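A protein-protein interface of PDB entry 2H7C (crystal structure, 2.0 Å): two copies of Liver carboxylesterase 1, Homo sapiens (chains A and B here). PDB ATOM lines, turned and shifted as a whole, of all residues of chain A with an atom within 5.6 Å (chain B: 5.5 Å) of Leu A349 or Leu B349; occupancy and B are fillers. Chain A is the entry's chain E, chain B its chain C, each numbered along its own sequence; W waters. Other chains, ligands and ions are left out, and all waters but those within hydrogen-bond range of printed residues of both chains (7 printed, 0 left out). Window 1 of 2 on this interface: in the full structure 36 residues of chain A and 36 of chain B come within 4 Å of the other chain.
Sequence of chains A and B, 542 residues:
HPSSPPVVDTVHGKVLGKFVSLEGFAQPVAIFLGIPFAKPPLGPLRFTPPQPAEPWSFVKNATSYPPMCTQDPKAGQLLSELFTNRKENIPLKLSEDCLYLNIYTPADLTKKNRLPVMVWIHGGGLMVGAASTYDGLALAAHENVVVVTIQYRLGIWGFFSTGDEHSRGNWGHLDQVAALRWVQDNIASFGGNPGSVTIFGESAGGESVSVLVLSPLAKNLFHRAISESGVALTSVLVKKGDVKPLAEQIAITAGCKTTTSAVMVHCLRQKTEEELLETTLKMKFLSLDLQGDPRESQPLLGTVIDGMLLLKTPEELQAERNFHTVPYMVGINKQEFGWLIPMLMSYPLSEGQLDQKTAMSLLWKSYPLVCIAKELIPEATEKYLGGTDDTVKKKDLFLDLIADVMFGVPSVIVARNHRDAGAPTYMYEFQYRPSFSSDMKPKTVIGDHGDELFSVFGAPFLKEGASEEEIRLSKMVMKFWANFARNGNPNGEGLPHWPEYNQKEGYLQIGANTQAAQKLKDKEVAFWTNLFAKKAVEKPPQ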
ATOM      1  N   TRP A 339      -6.614   2.422   5.131  1.00  0.00           N
ATOM      2  CA  TRP A 339      -7.143   2.296   3.781  1.00  0.00           C
ATOM      3  C   TRP A 339      -8.314   3.220   3.455  1.00  0.00           C
ATOM      4  O   TRP A 339      -8.240   4.000   2.514  1.00  0.00           O
ATOM      5  CB  TRP A 339      -7.583   0.851   3.525  1.00  0.00           C
ATOM      6  CG  TRP A 339      -8.053   0.610   2.118  1.00  0.00           C
ATOM      7  CD1 TRP A 339      -7.273   0.466   1.006  1.00  0.00           C
ATOM      8  CD2 TRP A 339      -9.412   0.506   1.669  1.00  0.00           C
ATOM      9  NE1 TRP A 339      -8.059   0.276  -0.106  1.00  0.00           N
ATOM     10  CE2 TRP A 339      -9.377   0.298   0.271  1.00  0.00           C
ATOM     11  CE3 TRP A 339     -10.657   0.571   2.313  1.00  0.00           C
ATOM     12  CZ2 TRP A 339     -10.540   0.153  -0.497  1.00  0.00           C
ATOM     13  CZ3 TRP A 339     -11.817   0.426   1.548  1.00  0.00           C
ATOM     14  CH2 TRP A 339     -11.746   0.219   0.156  1.00  0.00           C
ATOM     15  N   PRO A 342      -7.519   7.272   3.314  1.00  0.00           N
ATOM     16  CA  PRO A 342      -6.602   7.561   2.201  1.00  0.00           C
ATOM     17  C   PRO A 342      -7.305   7.346   0.858  1.00  0.00           C
ATOM     18  O   PRO A 342      -7.100   8.097  -0.099  1.00  0.00           O
ATOM     19  CB  PRO A 342      -5.471   6.551   2.407  1.00  0.00           C
ATOM     20  CG  PRO A 342      -5.476   6.320   3.879  1.00  0.00           C
ATOM     21  CD  PRO A 342      -6.935   6.279   4.235  1.00  0.00           C
ATOM     22  N   TYR A 347      -5.636   9.989  -1.586  1.00  0.00           N
ATOM     23  CA  TYR A 347      -4.262  10.126  -1.122  1.00  0.00           C
ATOM     24  C   TYR A 347      -3.325   9.498  -2.154  1.00  0.00           C
ATOM     25  O   TYR A 347      -3.542   8.370  -2.594  1.00  0.00           O
ATOM     26  CB  TYR A 347      -4.101   9.427   0.227  1.00  0.00           C
ATOM     27  CG  TYR A 347      -3.042  10.038   1.109  1.00  0.00           C
ATOM     28  CD1 TYR A 347      -3.256  11.259   1.746  1.00  0.00           C
ATOM     29  CD2 TYR A 347      -1.820   9.399   1.303  1.00  0.00           C
ATOM     30  CE1 TYR A 347      -2.277  11.827   2.556  1.00  0.00           C
ATOM     31  CE2 TYR A 347      -0.836   9.956   2.107  1.00  0.00           C
ATOM     32  CZ  TYR A 347      -1.067  11.167   2.730  1.00  0.00           C
ATOM     33  OH  TYR A 347      -0.082  11.710   3.524  1.00  0.00           O
ATOM     34  N   PRO A 348      -2.271  10.227  -2.558  1.00  0.00           N
ATOM     35  CA  PRO A 348      -1.289   9.762  -3.545  1.00  0.00           C
ATOM     36  C   PRO A 348      -0.358   8.662  -3.035  1.00  0.00           C
ATOM     37  O   PRO A 348       0.735   8.953  -2.554  1.00  0.00           O
ATOM     38  CB  PRO A 348      -0.507  11.034  -3.886  1.00  0.00           C
ATOM     39  CG  PRO A 348      -1.434  12.146  -3.498  1.00  0.00           C
ATOM     40  CD  PRO A 348      -2.032  11.639  -2.225  1.00  0.00           C
ATOM     41  N   LEU A 349      -0.782   7.405  -3.151  1.00  0.00           N
ATOM     42  CA  LEU A 349       0.038   6.285  -2.697  1.00  0.00           C
ATOM     43  C   LEU A 349      -0.013   5.081  -3.635  1.00  0.00           C
ATOM     44  O   LEU A 349       0.089   3.935  -3.195  1.00  0.00           O
ATOM     45  CB  LEU A 349      -0.387   5.858  -1.292  1.00  0.00           C
ATOM     46  CG  LEU A 349      -0.023   6.809  -0.151  1.00  0.00           C
ATOM     47  CD1 LEU A 349      -0.601   6.282   1.151  1.00  0.00           C
ATOM     48  CD2 LEU A 349       1.489   6.939  -0.050  1.00  0.00           C
ATOM     49  N   SER A 350      -0.163   5.348  -4.928  1.00  0.00           N
ATOM     50  CA  SER A 350      -0.226   4.295  -5.936  1.00  0.00           C
ATOM     51  C   SER A 350       0.793   3.196  -5.648  1.00  0.00           C
ATOM     52  O   SER A 350       0.435   2.032  -5.477  1.00  0.00           O
ATOM     53  CB  SER A 350       0.039   4.883  -7.327  1.00  0.00           C
ATOM     54  OG  SER A 350      -0.828   5.971  -7.599  1.00  0.00           O
ATOM     55  N   GLU A 351       2.066   3.573  -5.596  1.00  0.00           N
ATOM     56  CA  GLU A 351       3.132   2.616  -5.333  1.00  0.00           C
ATOM     57  C   GLU A 351       3.041   2.030  -3.936  1.00  0.00           C
ATOM     58  O   GLU A 351       2.173   2.404  -3.150  1.00  0.00           O
ATOM     59  CB  GLU A 351       4.495   3.279  -5.527  1.00  0.00           C
ATOM     60  CG  GLU A 351       4.829   3.533  -6.982  1.00  0.00           C
ATOM     61  CD  GLU A 351       4.996   2.246  -7.767  1.00  0.00           C
ATOM     62  OE1 GLU A 351       5.914   1.467  -7.436  1.00  0.00           O
ATOM     63  OE2 GLU A 351       4.209   2.011  -8.710  1.00  0.00           O
ATOM     64  N   GLY A 352       3.942   1.100  -3.637  1.00  0.00           N
ATOM     65  CA  GLY A 352       3.947   0.472  -2.332  1.00  0.00           C
ATOM     66  C   GLY A 352       4.952   1.101  -1.390  1.00  0.00           C
ATOM     67  O   GLY A 352       4.602   1.990  -0.615  1.00  0.00           O
ATOM     68  N   LEU A 354       8.017   3.269   0.294  1.00  0.00           N
ATOM     69  CA  LEU A 354       8.194   4.714   0.316  1.00  0.00           C
ATOM     70  C   LEU A 354       9.521   5.165   0.921  1.00  0.00           C
ATOM     71  O   LEU A 354       9.918   4.695   1.985  1.00  0.00           O
ATOM     72  CB  LEU A 354       7.042   5.335   1.110  1.00  0.00           C
ATOM     73  CG  LEU A 354       6.936   6.855   1.205  1.00  0.00           C
ATOM     74  CD1 LEU A 354       6.595   7.425  -0.161  1.00  0.00           C
ATOM     75  CD2 LEU A 354       5.857   7.226   2.213  1.00  0.00           C
ATOM     76  N   LEU A 362       5.129  14.220   1.027  1.00  0.00           N
ATOM     77  CA  LEU A 362       3.739  13.835   1.238  1.00  0.00           C
ATOM     78  C   LEU A 362       3.211  14.402   2.552  1.00  0.00           C
ATOM     79  O   LEU A 362       2.067  14.854   2.628  1.00  0.00           O
ATOM     80  CB  LEU A 362       3.597  12.311   1.266  1.00  0.00           C
ATOM     81  CG  LEU A 362       3.516  11.563  -0.068  1.00  0.00           C
ATOM     82  CD1 LEU A 362       3.438  10.071   0.198  1.00  0.00           C
ATOM     83  CD2 LEU A 362       2.296  12.031  -0.849  1.00  0.00           C
ATOM     84  N   LYS A 395       6.496   2.871   4.607  1.00  0.00           N
ATOM     85  CA  LYS A 395       5.179   3.240   4.113  1.00  0.00           C
ATOM     86  C   LYS A 395       4.152   2.898   5.190  1.00  0.00           C
ATOM     87  O   LYS A 395       3.216   3.656   5.434  1.00  0.00           O
ATOM     88  CB  LYS A 395       4.890   2.490   2.806  1.00  0.00           C
ATOM     89  CG  LYS A 395       3.434   2.468   2.377  1.00  0.00           C
ATOM     90  CD  LYS A 395       2.689   1.357   3.095  1.00  0.00           C
ATOM     91  CE  LYS A 395       1.205   1.409   2.815  1.00  0.00           C
ATOM     92  NZ  LYS A 395       0.482   0.378   3.611  1.00  0.00           N
ATOM     93  N   PHE A 398       4.628   5.260   7.924  1.00  0.00           N
ATOM     94  CA  PHE A 398       4.148   6.571   7.518  1.00  0.00           C
ATOM     95  C   PHE A 398       2.653   6.672   7.807  1.00  0.00           C
ATOM     96  O   PHE A 398       2.165   7.702   8.267  1.00  0.00           O
ATOM     97  CB  PHE A 398       4.395   6.801   6.026  1.00  0.00           C
ATOM     98  CG  PHE A 398       4.028   8.179   5.571  1.00  0.00           C
ATOM     99  CD1 PHE A 398       4.809   9.272   5.932  1.00  0.00           C
ATOM    100  CD2 PHE A 398       2.872   8.397   4.827  1.00  0.00           C
ATOM    101  CE1 PHE A 398       4.446  10.567   5.560  1.00  0.00           C
ATOM    102  CE2 PHE A 398       2.499   9.688   4.449  1.00  0.00           C
ATOM    103  CZ  PHE A 398       3.288  10.773   4.818  1.00  0.00           C
ATOM    104  N   LEU A 399       1.924   5.595   7.537  1.00  0.00           N
ATOM    105  CA  LEU A 399       0.487   5.585   7.784  1.00  0.00           C
ATOM    106  C   LEU A 399       0.197   5.610   9.284  1.00  0.00           C
ATOM    107  O   LEU A 399      -0.839   6.115   9.709  1.00  0.00           O
ATOM    108  CB  LEU A 399      -0.151   4.352   7.139  1.00  0.00           C
ATOM    109  CG  LEU A 399       0.003   4.241   5.619  1.00  0.00           C
ATOM    110  CD1 LEU A 399      -0.650   2.950   5.133  1.00  0.00           C
ATOM    111  CD2 LEU A 399      -0.635   5.456   4.947  1.00  0.00           C
ATOM    112  N   TRP B 339       2.392   5.518 -11.598  1.00  0.00           N
ATOM    113  CA  TRP B 339       2.052   6.473 -10.550  1.00  0.00           C
ATOM    114  C   TRP B 339       1.094   7.583 -10.972  1.00  0.00           C
ATOM    115  O   TRP B 339       0.027   7.742 -10.394  1.00  0.00           O
ATOM    116  CB  TRP B 339       3.327   7.118 -10.001  1.00  0.00           C
ATOM    117  CG  TRP B 339       3.079   8.063  -8.858  1.00  0.00           C
ATOM    118  CD1 TRP B 339       2.856   7.729  -7.553  1.00  0.00           C
ATOM    119  CD2 TRP B 339       2.983   9.494  -8.927  1.00  0.00           C
ATOM    120  NE1 TRP B 339       2.627   8.861  -6.806  1.00  0.00           N
ATOM    121  CE2 TRP B 339       2.699   9.958  -7.623  1.00  0.00           C
ATOM    122  CE3 TRP B 339       3.108  10.429  -9.966  1.00  0.00           C
ATOM    123  CZ2 TRP B 339       2.537  11.318  -7.327  1.00  0.00           C
ATOM    124  CZ3 TRP B 339       2.946  11.785  -9.672  1.00  0.00           C
ATOM    125  CH2 TRP B 339       2.664  12.213  -8.360  1.00  0.00           C
ATOM    126  N   PRO B 342      -2.707   6.461 -12.009  1.00  0.00           N
ATOM    127  CA  PRO B 342      -3.455   5.962 -10.850  1.00  0.00           C
ATOM    128  C   PRO B 342      -3.704   7.086  -9.840  1.00  0.00           C
ATOM    129  O   PRO B 342      -4.735   7.120  -9.168  1.00  0.00           O
ATOM    130  CB  PRO B 342      -2.537   4.880 -10.284  1.00  0.00           C
ATOM    131  CG  PRO B 342      -1.797   4.391 -11.495  1.00  0.00           C
ATOM    132  CD  PRO B 342      -1.486   5.666 -12.233  1.00  0.00           C
ATOM    133  N   TYR B 347      -7.023   6.046  -7.896  1.00  0.00           N
ATOM    134  CA  TYR B 347      -7.045   4.594  -7.757  1.00  0.00           C
ATOM    135  C   TYR B 347      -6.821   4.210  -6.300  1.00  0.00           C
ATOM    136  O   TYR B 347      -6.017   4.827  -5.610  1.00  0.00           O
ATOM    137  CB  TYR B 347      -5.952   3.953  -8.610  1.00  0.00           C
ATOM    138  CG  TYR B 347      -6.491   3.168  -9.774  1.00  0.00           C
ATOM    139  CD1 TYR B 347      -7.149   3.810 -10.820  1.00  0.00           C
ATOM    140  CD2 TYR B 347      -6.364   1.782  -9.824  1.00  0.00           C
ATOM    141  CE1 TYR B 347      -7.666   3.094 -11.885  1.00  0.00           C
ATOM    142  CE2 TYR B 347      -6.880   1.055 -10.888  1.00  0.00           C
ATOM    143  CZ  TYR B 347      -7.530   1.722 -11.914  1.00  0.00           C
ATOM    144  OH  TYR B 347      -8.045   1.020 -12.977  1.00  0.00           O
ATOM    145  N   PRO B 348      -7.546   3.191  -5.812  1.00  0.00           N
ATOM    146  CA  PRO B 348      -7.422   2.722  -4.425  1.00  0.00           C
ATOM    147  C   PRO B 348      -6.197   1.820  -4.241  1.00  0.00           C
ATOM    148  O   PRO B 348      -6.261   0.628  -4.539  1.00  0.00           O
ATOM    149  CB  PRO B 348      -8.721   1.942  -4.201  1.00  0.00           C
ATOM    150  CG  PRO B 348      -9.648   2.447  -5.271  1.00  0.00           C
ATOM    151  CD  PRO B 348      -8.738   2.611  -6.447  1.00  0.00           C
ATOM    152  N   LEU B 349      -5.096   2.378  -3.743  1.00  0.00           N
ATOM    153  CA  LEU B 349      -3.873   1.598  -3.542  1.00  0.00           C
ATOM    154  C   LEU B 349      -2.998   2.114  -2.397  1.00  0.00           C
ATOM    155  O   LEU B 349      -1.776   2.174  -2.519  1.00  0.00           O
ATOM    156  CB  LEU B 349      -3.058   1.581  -4.837  1.00  0.00           C
ATOM    157  CG  LEU B 349      -3.687   0.862  -6.034  1.00  0.00           C
ATOM    158  CD1 LEU B 349      -2.864   1.132  -7.282  1.00  0.00           C
ATOM    159  CD2 LEU B 349      -3.770  -0.631  -5.755  1.00  0.00           C
ATOM    160  N   SER B 350      -3.626   2.461  -1.281  1.00  0.00           N
ATOM    161  CA  SER B 350      -2.910   2.987  -0.122  1.00  0.00           C
ATOM    162  C   SER B 350      -1.877   2.038   0.493  1.00  0.00           C
ATOM    163  O   SER B 350      -0.749   2.441   0.772  1.00  0.00           O
ATOM    164  CB  SER B 350      -3.912   3.397   0.963  1.00  0.00           C
ATOM    165  OG  SER B 350      -4.892   4.286   0.453  1.00  0.00           O
ATOM    166  N   GLU B 351      -2.261   0.783   0.700  1.00  0.00           N
ATOM    167  CA  GLU B 351      -1.380  -0.201   1.324  1.00  0.00           C
ATOM    168  C   GLU B 351      -0.114  -0.621   0.579  1.00  0.00           C
ATOM    169  O   GLU B 351       0.857  -1.045   1.209  1.00  0.00           O
ATOM    170  CB  GLU B 351      -2.180  -1.446   1.698  1.00  0.00           C
ATOM    171  CG  GLU B 351      -3.050  -1.244   2.924  1.00  0.00           C
ATOM    172  CD  GLU B 351      -2.234  -0.899   4.159  1.00  0.00           C
ATOM    173  OE1 GLU B 351      -1.279  -1.644   4.463  1.00  0.00           O
ATOM    174  OE2 GLU B 351      -2.550   0.107   4.830  1.00  0.00           O
ATOM    175  N   GLY B 352      -0.115  -0.521  -0.746  1.00  0.00           N
ATOM    176  CA  GLY B 352       1.070  -0.893  -1.499  1.00  0.00           C
ATOM    177  C   GLY B 352       1.215  -2.382  -1.754  1.00  0.00           C
ATOM    178  O   GLY B 352       1.977  -2.793  -2.625  1.00  0.00           O
ATOM    179  N   LEU B 354      -0.872  -6.322  -2.222  1.00  0.00           N
ATOM    180  CA  LEU B 354      -2.073  -6.761  -2.918  1.00  0.00           C
ATOM    181  C   LEU B 354      -2.182  -8.267  -3.100  1.00  0.00           C
ATOM    182  O   LEU B 354      -1.329  -8.892  -3.722  1.00  0.00           O
ATOM    183  CB  LEU B 354      -2.133  -6.083  -4.289  1.00  0.00           C
ATOM    184  CG  LEU B 354      -3.441  -6.169  -5.074  1.00  0.00           C
ATOM    185  CD1 LEU B 354      -4.498  -5.294  -4.412  1.00  0.00           C
ATOM    186  CD2 LEU B 354      -3.202  -5.708  -6.498  1.00  0.00           C
ATOM    187  N   LEU B 362     -10.250  -5.124  -8.122  1.00  0.00           N
ATOM    188  CA  LEU B 362      -9.808  -3.864  -8.697  1.00  0.00           C
ATOM    189  C   LEU B 362      -9.828  -3.929 -10.224  1.00  0.00           C
ATOM    190  O   LEU B 362     -10.182  -2.953 -10.884  1.00  0.00           O
ATOM    191  CB  LEU B 362      -8.395  -3.522  -8.211  1.00  0.00           C
ATOM    192  CG  LEU B 362      -8.229  -3.100  -6.749  1.00  0.00           C
ATOM    193  CD1 LEU B 362      -6.746  -2.859  -6.460  1.00  0.00           C
ATOM    194  CD2 LEU B 362      -9.033  -1.832  -6.474  1.00  0.00           C
ATOM    195  N   LYS B 395       1.276  -6.394  -6.537  1.00  0.00           N
ATOM    196  CA  LYS B 395       0.666  -5.116  -6.866  1.00  0.00           C
ATOM    197  C   LYS B 395       1.465  -4.459  -7.988  1.00  0.00           C
ATOM    198  O   LYS B 395       0.917  -3.713  -8.797  1.00  0.00           O
ATOM    199  CB  LYS B 395       0.618  -4.214  -5.627  1.00  0.00           C
ATOM    200  CG  LYS B 395       1.793  -3.270  -5.464  1.00  0.00           C
ATOM    201  CD  LYS B 395       1.549  -1.971  -6.205  1.00  0.00           C
ATOM    202  CE  LYS B 395       2.709  -1.011  -6.024  1.00  0.00           C
ATOM    203  NZ  LYS B 395       2.497   0.251  -6.780  1.00  0.00           N
ATOM    204  N   PHE B 398       0.495  -6.072 -11.018  1.00  0.00           N
ATOM    205  CA  PHE B 398      -0.863  -5.630 -11.294  1.00  0.00           C
ATOM    206  C   PHE B 398      -0.813  -4.344 -12.122  1.00  0.00           C
ATOM    207  O   PHE B 398      -1.607  -4.154 -13.039  1.00  0.00           O
ATOM    208  CB  PHE B 398      -1.612  -5.382  -9.982  1.00  0.00           C
ATOM    209  CG  PHE B 398      -3.012  -4.871 -10.171  1.00  0.00           C
ATOM    210  CD1 PHE B 398      -4.000  -5.692 -10.703  1.00  0.00           C
ATOM    211  CD2 PHE B 398      -3.337  -3.562  -9.840  1.00  0.00           C
ATOM    212  CE1 PHE B 398      -5.294  -5.214 -10.907  1.00  0.00           C
ATOM    213  CE2 PHE B 398      -4.628  -3.075 -10.042  1.00  0.00           C
ATOM    214  CZ  PHE B 398      -5.606  -3.905 -10.576  1.00  0.00           C
ATOM    215  N   LEU B 399       0.126  -3.463 -11.792  1.00  0.00           N
ATOM    216  CA  LEU B 399       0.278  -2.205 -12.515  1.00  0.00           C
ATOM    217  C   LEU B 399       0.814  -2.481 -13.922  1.00  0.00           C
ATOM    218  O   LEU B 399       0.481  -1.767 -14.873  1.00  0.00           O
ATOM    219  CB  LEU B 399       1.213  -1.258 -11.750  1.00  0.00           C
ATOM    220  CG  LEU B 399       0.750  -0.840 -10.343  1.00  0.00           C
ATOM    221  CD1 LEU B 399       1.825   0.017  -9.685  1.00  0.00           C
ATOM    222  CD2 LEU B 399      -0.564  -0.071 -10.419  1.00  0.00           C
HETATM  223  O   HOH W   1      -3.129   5.941  -6.361  1.00  0.00           O
HETATM  224  O   HOH W   2       3.405   8.768  -3.441  1.00  0.00           O
HETATM  225  O   HOH W   3       4.795  -2.060  -4.265  1.00  0.00           O
HETATM  226  O   HOH W   4      -5.409   6.204  -1.730  1.00  0.00           O
HETATM  227  O   HOH W   5      -5.085   7.461  -5.411  1.00  0.00           O
HETATM  228  O   HOH W   6      -3.516   5.211  -3.738  1.00  0.00           O
HETATM  229  O   HOH W   7      -6.839  -1.453  -2.533  1.00  0.00           O
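Water W1 lies within hydrogen-bond range of the side-chain hydroxyl (OG) of Ser A350 (2.6 Å), the backbone carbonyl oxygen (O) of Tyr B347 (3.2 Å) and the backbone carbonyl oxygen (O) of Pro B342 (3.4 Å).
Water W5 bridges the backbone carbonyl oxygen of Tyr B347 (2.8 Å) and the backbone carbonyl oxygen of Tyr A347 (3.3 Å).
Water W2 lies within hydrogen-bond range of the backbone carbonyl oxygen of Pro A348 (2.8 Å) and the indole nitrogen of Trp B339 (3.5 Å).
Water W7 lies within hydrogen-bond range of the backbone carbonyl oxygen of Pro B348 and the indole nitrogen of Trp A339.
Water W6 lies within hydrogen-bond range of O of Tyr B347 (3.1 Å), N of Leu B349 (3.2 Å) and O of Tyr A347 (3.4 Å).
Water W3 bridges N of Gly A352 (3.3 Å) and O of Gly B352 (3.3 Å).
Leu A349 touches Ser B350, and with the chains exchanged Ser A350 touches Leu B349.
Glu A351 touches Gly B352, but with the chains exchanged Gly A352 does not touch Glu B351 (4.9 Å).
Glu A351 touches Lys B395, and with the chains exchanged Lys A395 touches Glu B351.
Gly A352 touches Lys B395, but with the chains exchanged Lys A395 does not touch Gly B352 (4.3 Å).
Positions printed for both chains: 339, 342, 347, 348, 349, 350, 351, 352, 354, 362, 395, 398 and 399.
Of the 13 printed residues of chain B, 8 touch a printed residue of chain A.
Among the printed residues, Asp or Glu carboxylates within 4 Å of a Lys or Arg side-chain nitrogen of the other chain: Glu A351 with Lys B395 (3.1 Å) and Lys A395 with Glu B351 (2.8 Å).
The backbone carbonyl oxygen (O) of Pro A342 lies within hydrogen-bond range of the backbone NH (N) of Tyr A347, at 2.8 Å.
The backbone carbonyl oxygen (O) of Pro B342 sits at hydrogen-bond distance from the backbone NH (N) of Tyr B347 (2.8 Å).
Leu A349 touches just these residues of chain B: Leu B349 (2.7 Å) and Ser B350 (3.9 Å).
Of the printed residues of chain A, Leu B349 touches Leu A349 (2.7 Å) and Ser A350 (3.6 Å).
Of the printed residues of chain B, Glu A351 touches Gly B352, Lys B395 and Leu B399.
Of the printed residues of chain B, Trp A339 touches Ser B350.
Pro B348 touches none of the printed residues of chain A.
Leu B362 touches none of the printed residues of chain A.
The nearest residue of chain B that does not touch Leu A349 is Gly B352 (5.1 Å).
Among the printed residues, merely in contact across the chains: Lys A395 with Ser B350 (3.0 Å), Pro A342 with Ser B350 (3.0 Å), Glu A351 with Leu B399 (3.3 Å), Gly A352 with Gly B352 (3.3 Å), Ser A350 with Pro B342 (3.4 Å), Gly A352 with Lys B395 (3.4 Å), Leu A399 with Glu B351 (3.4 Å), Ser A350 with Leu B349 (3.6 Å), Glu A351 with Gly B352 (3.8 Å), Leu A349 with Ser B350 (3.9 Å) and Trp A339 with Ser B350 (3.9 Å).
OE1 of Glu B351 lies within salt-bridge range of NZ of Lys A395 (2.8 Å).
The backbone carbonyl oxygen of Trp B339 lies within hydrogen-bond range of the side-chain hydroxyl of Ser A350, at 3.4 Å.
O of Ser A350 lies within hydrogen-bond range of NZ of Lys B395 (3.0 Å).
NZ of Lys B395 is in salt-bridge range of OE2 of Glu A351 (3.1 Å).
O of Leu A349 lies close to O of Leu B349 (2.7 Å).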
